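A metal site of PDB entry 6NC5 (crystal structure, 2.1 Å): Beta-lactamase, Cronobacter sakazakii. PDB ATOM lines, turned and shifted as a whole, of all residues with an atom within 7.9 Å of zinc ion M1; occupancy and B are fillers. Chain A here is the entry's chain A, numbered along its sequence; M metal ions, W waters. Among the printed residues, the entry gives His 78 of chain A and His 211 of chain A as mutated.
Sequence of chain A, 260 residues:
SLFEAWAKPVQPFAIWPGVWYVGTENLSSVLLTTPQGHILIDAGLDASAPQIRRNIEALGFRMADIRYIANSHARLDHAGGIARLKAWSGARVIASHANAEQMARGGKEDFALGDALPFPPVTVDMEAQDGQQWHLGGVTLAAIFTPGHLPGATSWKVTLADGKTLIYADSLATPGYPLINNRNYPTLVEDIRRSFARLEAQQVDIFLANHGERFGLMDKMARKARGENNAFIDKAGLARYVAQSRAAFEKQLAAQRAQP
Zinc ion M1 is bound by the side-chain carboxylate of Asp 77 (2.0 Å), a ring nitrogen (NE2) of His 78 (2.0 Å), a ring nitrogen (NE2) of His 211 (2.0 Å) and water W1 (2.1 Å).
O of Asn 26 lies within hydrogen-bond range of ND1 of His 211. OD1 of Asp 170 sits at hydrogen-bond distance from ND1 of His 73 (2.6 Å).
Residues that only touch zinc ion M1: His 73 (3.9 Å). Four residues have an atom within 4 Å of zinc ion M1: His 73, Asp 77, His 78 and His 211. The nearest printed residue that does not touch zinc ion M1 is Asn 210 (4.8 Å).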
ATOM      1  N   PHE A   3      20.874   4.369  -3.536  1.00  0.00           N
ATOM      2  CA  PHE A   3      21.669   3.145  -3.488  1.00  0.00           C
ATOM      3  C   PHE A   3      21.614   2.396  -4.814  1.00  0.00           C
ATOM      4  O   PHE A   3      22.591   1.752  -5.204  1.00  0.00           O
ATOM      5  CB  PHE A   3      21.187   2.245  -2.352  1.00  0.00           C
ATOM      6  CG  PHE A   3      21.393   2.830  -0.985  1.00  0.00           C
ATOM      7  CD1 PHE A   3      22.586   3.447  -0.653  1.00  0.00           C
ATOM      8  CD2 PHE A   3      20.391   2.755  -0.030  1.00  0.00           C
ATOM      9  CE1 PHE A   3      22.777   3.988   0.605  1.00  0.00           C
ATOM     10  CE2 PHE A   3      20.579   3.289   1.235  1.00  0.00           C
ATOM     11  CZ  PHE A   3      21.775   3.902   1.551  1.00  0.00           C
ATOM     12  N   TRP A   6      24.123   4.087  -6.816  1.00  0.00           N
ATOM     13  CA  TRP A   6      25.435   3.755  -6.283  1.00  0.00           C
ATOM     14  C   TRP A   6      25.843   2.330  -6.650  1.00  0.00           C
ATOM     15  O   TRP A   6      27.043   2.050  -6.791  1.00  0.00           O
ATOM     16  CB  TRP A   6      25.439   3.916  -4.760  1.00  0.00           C
ATOM     17  CG  TRP A   6      25.550   5.333  -4.284  1.00  0.00           C
ATOM     18  CD1 TRP A   6      25.664   6.454  -5.063  1.00  0.00           C
ATOM     19  CD2 TRP A   6      25.551   5.790  -2.931  1.00  0.00           C
ATOM     20  NE1 TRP A   6      25.740   7.575  -4.275  1.00  0.00           N
ATOM     21  CE2 TRP A   6      25.677   7.195  -2.958  1.00  0.00           C
ATOM     22  CE3 TRP A   6      25.467   5.142  -1.692  1.00  0.00           C
ATOM     23  CZ2 TRP A   6      25.720   7.962  -1.796  1.00  0.00           C
ATOM     24  CZ3 TRP A   6      25.513   5.916  -0.537  1.00  0.00           C
ATOM     25  CH2 TRP A   6      25.638   7.303  -0.597  1.00  0.00           C
ATOM     26  N   ASN A  26      29.866   3.455  -7.185  1.00  0.00           N
ATOM     27  CA  ASN A  26      30.196   4.297  -6.040  1.00  0.00           C
ATOM     28  C   ASN A  26      30.308   3.533  -4.725  1.00  0.00           C
ATOM     29  O   ASN A  26      30.470   4.172  -3.677  1.00  0.00           O
ATOM     30  CB  ASN A  26      29.156   5.421  -5.886  1.00  0.00           C
ATOM     31  CG  ASN A  26      29.664   6.573  -5.048  1.00  0.00           C
ATOM     32  OD1 ASN A  26      30.768   7.071  -5.267  1.00  0.00           O
ATOM     33  ND2 ASN A  26      28.857   7.007  -4.081  1.00  0.00           N
ATOM     34  N   LEU A  27      30.224   2.212  -4.743  1.00  0.00           N
ATOM     35  CA  LEU A  27      30.410   1.408  -3.535  1.00  0.00           C
ATOM     36  C   LEU A  27      31.606   0.494  -3.766  1.00  0.00           C
ATOM     37  O   LEU A  27      31.533  -0.440  -4.577  1.00  0.00           O
ATOM     38  CB  LEU A  27      29.147   0.607  -3.212  1.00  0.00           C
ATOM     39  CG  LEU A  27      27.923   1.462  -2.889  1.00  0.00           C
ATOM     40  CD1 LEU A  27      26.722   0.577  -2.606  1.00  0.00           C
ATOM     41  CD2 LEU A  27      28.183   2.404  -1.722  1.00  0.00           C
ATOM     42  N   SER A  28      32.702   0.766  -3.065  1.00  0.00           N
ATOM     43  CA  SER A  28      33.965   0.106  -3.344  1.00  0.00           C
ATOM     44  C   SER A  28      33.995  -1.319  -2.810  1.00  0.00           C
ATOM     45  O   SER A  28      33.369  -1.646  -1.797  1.00  0.00           O
ATOM     46  CB  SER A  28      35.113   0.908  -2.748  1.00  0.00           C
ATOM     47  OG  SER A  28      35.159   2.217  -3.287  1.00  0.00           O
ATOM     48  N   ASP A  42      35.531  -4.901   2.141  1.00  0.00           N
ATOM     49  CA  ASP A  42      34.162  -4.427   1.970  1.00  0.00           C
ATOM     50  C   ASP A  42      33.427  -5.199   0.887  1.00  0.00           C
ATOM     51  O   ASP A  42      34.036  -5.824   0.025  1.00  0.00           O
ATOM     52  CB  ASP A  42      34.151  -2.931   1.661  1.00  0.00           C
ATOM     53  CG  ASP A  42      34.038  -2.080   2.907  1.00  0.00           C
ATOM     54  OD1 ASP A  42      33.659  -2.599   3.977  1.00  0.00           O
ATOM     55  OD2 ASP A  42      34.323  -0.865   2.826  1.00  0.00           O
ATOM     56  N   SER A  72      34.898  -1.885   6.595  1.00  0.00           N
ATOM     57  CA  SER A  72      35.213  -0.518   7.026  1.00  0.00           C
ATOM     58  C   SER A  72      34.262  -0.058   8.130  1.00  0.00           C
ATOM     59  O   SER A  72      34.696   0.224   9.246  1.00  0.00           O
ATOM     60  CB  SER A  72      35.149   0.433   5.826  1.00  0.00           C
ATOM     61  OG  SER A  72      33.913   0.324   5.147  1.00  0.00           O
ATOM     62  N   HIS A  73      32.963   0.019   7.838  1.00  0.00           N
ATOM     63  CA  HIS A  73      31.971   0.277   8.874  1.00  0.00           C
ATOM     64  C   HIS A  73      30.686  -0.475   8.544  1.00  0.00           C
ATOM     65  O   HIS A  73      30.405  -0.801   7.382  1.00  0.00           O
ATOM     66  CB  HIS A  73      31.708   1.788   9.067  1.00  0.00           C
ATOM     67  CG  HIS A  73      30.978   2.454   7.934  1.00  0.00           C
ATOM     68  ND1 HIS A  73      31.629   3.157   6.947  1.00  0.00           N
ATOM     69  CD2 HIS A  73      29.656   2.571   7.671  1.00  0.00           C
ATOM     70  CE1 HIS A  73      30.736   3.650   6.099  1.00  0.00           C
ATOM     71  NE2 HIS A  73      29.533   3.310   6.516  1.00  0.00           N
ATOM     72  N   ARG A  75      27.400  -0.568   8.027  1.00  0.00           N
ATOM     73  CA  ARG A  75      26.137  -0.137   7.465  1.00  0.00           C
ATOM     74  C   ARG A  75      25.922  -0.838   6.128  1.00  0.00           C
ATOM     75  O   ARG A  75      26.844  -1.407   5.551  1.00  0.00           O
ATOM     76  CB  ARG A  75      26.081   1.392   7.314  1.00  0.00           C
ATOM     77  CG  ARG A  75      25.666   2.077   8.601  1.00  0.00           C
ATOM     78  CD  ARG A  75      25.688   3.583   8.449  1.00  0.00           C
ATOM     79  NE  ARG A  75      25.331   4.264   9.683  1.00  0.00           N
ATOM     80  CZ  ARG A  75      25.523   5.557   9.914  1.00  0.00           C
ATOM     81  NH1 ARG A  75      26.074   6.313   8.977  1.00  0.00           N
ATOM     82  NH2 ARG A  75      25.161   6.098  11.069  1.00  0.00           N
ATOM     83  N   LEU A  76      24.681  -0.778   5.641  1.00  0.00           N
ATOM     84  CA  LEU A  76      24.270  -1.668   4.574  1.00  0.00           C
ATOM     85  C   LEU A  76      25.053  -1.459   3.284  1.00  0.00           C
ATOM     86  O   LEU A  76      25.200  -2.391   2.487  1.00  0.00           O
ATOM     87  CB  LEU A  76      22.769  -1.505   4.319  1.00  0.00           C
ATOM     88  CG  LEU A  76      22.307  -0.286   3.507  1.00  0.00           C
ATOM     89  CD1 LEU A  76      20.845  -0.482   3.111  1.00  0.00           C
ATOM     90  CD2 LEU A  76      22.484   1.000   4.282  1.00  0.00           C
ATOM     91  N   ASP A  77      25.551  -0.246   3.045  1.00  0.00           N
ATOM     92  CA  ASP A  77      26.240   0.019   1.782  1.00  0.00           C
ATOM     93  C   ASP A  77      27.677  -0.480   1.768  1.00  0.00           C
ATOM     94  O   ASP A  77      28.373  -0.283   0.764  1.00  0.00           O
ATOM     95  CB  ASP A  77      26.219   1.524   1.462  1.00  0.00           C
ATOM     96  CG  ASP A  77      26.798   2.379   2.571  1.00  0.00           C
ATOM     97  OD1 ASP A  77      26.797   1.951   3.738  1.00  0.00           O
ATOM     98  OD2 ASP A  77      27.276   3.494   2.258  1.00  0.00           O
ATOM     99  N   HIS A  78      28.130  -1.127   2.840  1.00  0.00           N
ATOM    100  CA  HIS A  78      29.453  -1.752   2.858  1.00  0.00           C
ATOM    101  C   HIS A  78      29.466  -3.131   3.487  1.00  0.00           C
ATOM    102  O   HIS A  78      30.279  -3.961   3.076  1.00  0.00           O
ATOM    103  CB  HIS A  78      30.443  -0.853   3.609  1.00  0.00           C
ATOM    104  CG  HIS A  78      30.439   0.569   3.142  1.00  0.00           C
ATOM    105  ND1 HIS A  78      31.079   0.976   1.993  1.00  0.00           N
ATOM    106  CD2 HIS A  78      29.849   1.675   3.659  1.00  0.00           C
ATOM    107  CE1 HIS A  78      30.896   2.276   1.827  1.00  0.00           C
ATOM    108  NE2 HIS A  78      30.151   2.721   2.818  1.00  0.00           N
ATOM    109  N   HIS A 149      32.312   8.693  11.777  1.00  0.00           N
ATOM    110  CA  HIS A 149      31.145   8.340  10.981  1.00  0.00           C
ATOM    111  C   HIS A 149      30.333   7.255  11.670  1.00  0.00           C
ATOM    112  O   HIS A 149      29.095   7.301  11.684  1.00  0.00           O
ATOM    113  CB  HIS A 149      31.603   7.891   9.591  1.00  0.00           C
ATOM    114  CG  HIS A 149      30.478   7.537   8.665  1.00  0.00           C
ATOM    115  ND1 HIS A 149      29.620   8.478   8.139  1.00  0.00           N
ATOM    116  CD2 HIS A 149      30.078   6.340   8.171  1.00  0.00           C
ATOM    117  CE1 HIS A 149      28.734   7.865   7.361  1.00  0.00           C
ATOM    118  NE2 HIS A 149      28.999   6.573   7.368  1.00  0.00           N
ATOM    119  N   ASP A 170      37.943   4.948   5.277  1.00  0.00           N
ATOM    120  CA  ASP A 170      36.526   4.941   5.613  1.00  0.00           C
ATOM    121  C   ASP A 170      35.953   6.344   5.474  1.00  0.00           C
ATOM    122  O   ASP A 170      36.674   7.339   5.360  1.00  0.00           O
ATOM    123  CB  ASP A 170      36.319   4.405   7.023  1.00  0.00           C
ATOM    124  CG  ASP A 170      34.942   3.791   7.212  1.00  0.00           C
ATOM    125  OD1 ASP A 170      33.993   4.222   6.528  1.00  0.00           O
ATOM    126  OD2 ASP A 170      34.803   2.865   8.051  1.00  0.00           O
ATOM    127  N   SER A 171      34.623   6.415   5.486  1.00  0.00           N
ATOM    128  CA  SER A 171      33.949   7.702   5.422  1.00  0.00           C
ATOM    129  C   SER A 171      34.179   8.493   6.706  1.00  0.00           C
ATOM    130  O   SER A 171      34.346   7.932   7.790  1.00  0.00           O
ATOM    131  CB  SER A 171      32.447   7.506   5.198  1.00  0.00           C
ATOM    132  OG  SER A 171      31.704   8.634   5.608  1.00  0.00           O
ATOM    133  N   ASN A 210      36.005   3.983   0.457  1.00  0.00           N
ATOM    134  CA  ASN A 210      34.869   3.080   0.268  1.00  0.00           C
ATOM    135  C   ASN A 210      33.754   3.687  -0.584  1.00  0.00           C
ATOM    136  O   ASN A 210      32.749   3.017  -0.824  1.00  0.00           O
ATOM    137  CB  ASN A 210      34.312   2.621   1.623  1.00  0.00           C
ATOM    138  CG  ASN A 210      33.908   3.766   2.525  1.00  0.00           C
ATOM    139  OD1 ASN A 210      33.896   4.928   2.126  1.00  0.00           O
ATOM    140  ND2 ASN A 210      33.559   3.431   3.773  1.00  0.00           N
ATOM    141  N   HIS A 211      33.916   4.920  -1.055  1.00  0.00           N
ATOM    142  CA  HIS A 211      32.993   5.535  -2.004  1.00  0.00           C
ATOM    143  C   HIS A 211      33.805   6.091  -3.164  1.00  0.00           C
ATOM    144  O   HIS A 211      34.711   6.905  -2.959  1.00  0.00           O
ATOM    145  CB  HIS A 211      32.154   6.628  -1.348  1.00  0.00           C
ATOM    146  CG  HIS A 211      31.019   6.100  -0.541  1.00  0.00           C
ATOM    147  ND1 HIS A 211      29.817   5.706  -1.100  1.00  0.00           N
ATOM    148  CD2 HIS A 211      30.893   5.881   0.788  1.00  0.00           C
ATOM    149  CE1 HIS A 211      29.004   5.281  -0.150  1.00  0.00           C
ATOM    150  NE2 HIS A 211      29.639   5.375   1.005  1.00  0.00           N
ATOM    151  N   GLU A 213      33.377   8.224  -5.564  1.00  0.00           N
ATOM    152  CA  GLU A 213      33.419   9.654  -5.840  1.00  0.00           C
ATOM    153  C   GLU A 213      34.482  10.375  -5.039  1.00  0.00           C
ATOM    154  O   GLU A 213      34.884  11.481  -5.409  1.00  0.00           O
ATOM    155  CB  GLU A 213      32.055  10.273  -5.545  1.00  0.00           C
ATOM    156  CG  GLU A 213      31.696  10.303  -4.065  1.00  0.00           C
ATOM    157  CD  GLU A 213      30.205  10.379  -3.813  1.00  0.00           C
ATOM    158  OE1 GLU A 213      29.728   9.749  -2.838  1.00  0.00           O
ATOM    159  OE2 GLU A 213      29.508  11.079  -4.576  1.00  0.00           O
ATOM    160  N   ARG A 214      34.969   9.774  -3.952  1.00  0.00           N
ATOM    161  CA  ARG A 214      35.882  10.450  -3.043  1.00  0.00           C
ATOM    162  C   ARG A 214      37.357  10.197  -3.357  1.00  0.00           C
ATOM    163  O   ARG A 214      38.216  10.860  -2.778  1.00  0.00           O
ATOM    164  CB  ARG A 214      35.592  10.039  -1.595  1.00  0.00           C
ATOM    165  CG  ARG A 214      34.388  10.756  -1.000  1.00  0.00           C
ATOM    166  CD  ARG A 214      33.863  10.048   0.230  1.00  0.00           C
ATOM    167  NE  ARG A 214      32.412  10.182   0.351  1.00  0.00           N
ATOM    168  CZ  ARG A 214      31.703   9.779   1.398  1.00  0.00           C
ATOM    169  NH1 ARG A 214      32.316   9.216   2.433  1.00  0.00           N
ATOM    170  NH2 ARG A 214      30.388   9.941   1.417  1.00  0.00           N
HETATM  171 ZN    ZN M   1      28.989   4.348   2.646  1.00  0.00          ZN
HETATM  172 ZN    ZN M   2      28.446   5.149   5.938  1.00  0.00          ZN
HETATM  173 ZN    ZN M   3      25.253   5.841   5.038  1.00  0.00          ZN
HETATM  174  O   HOH W   1      29.306   5.814   4.098  1.00  0.00           O
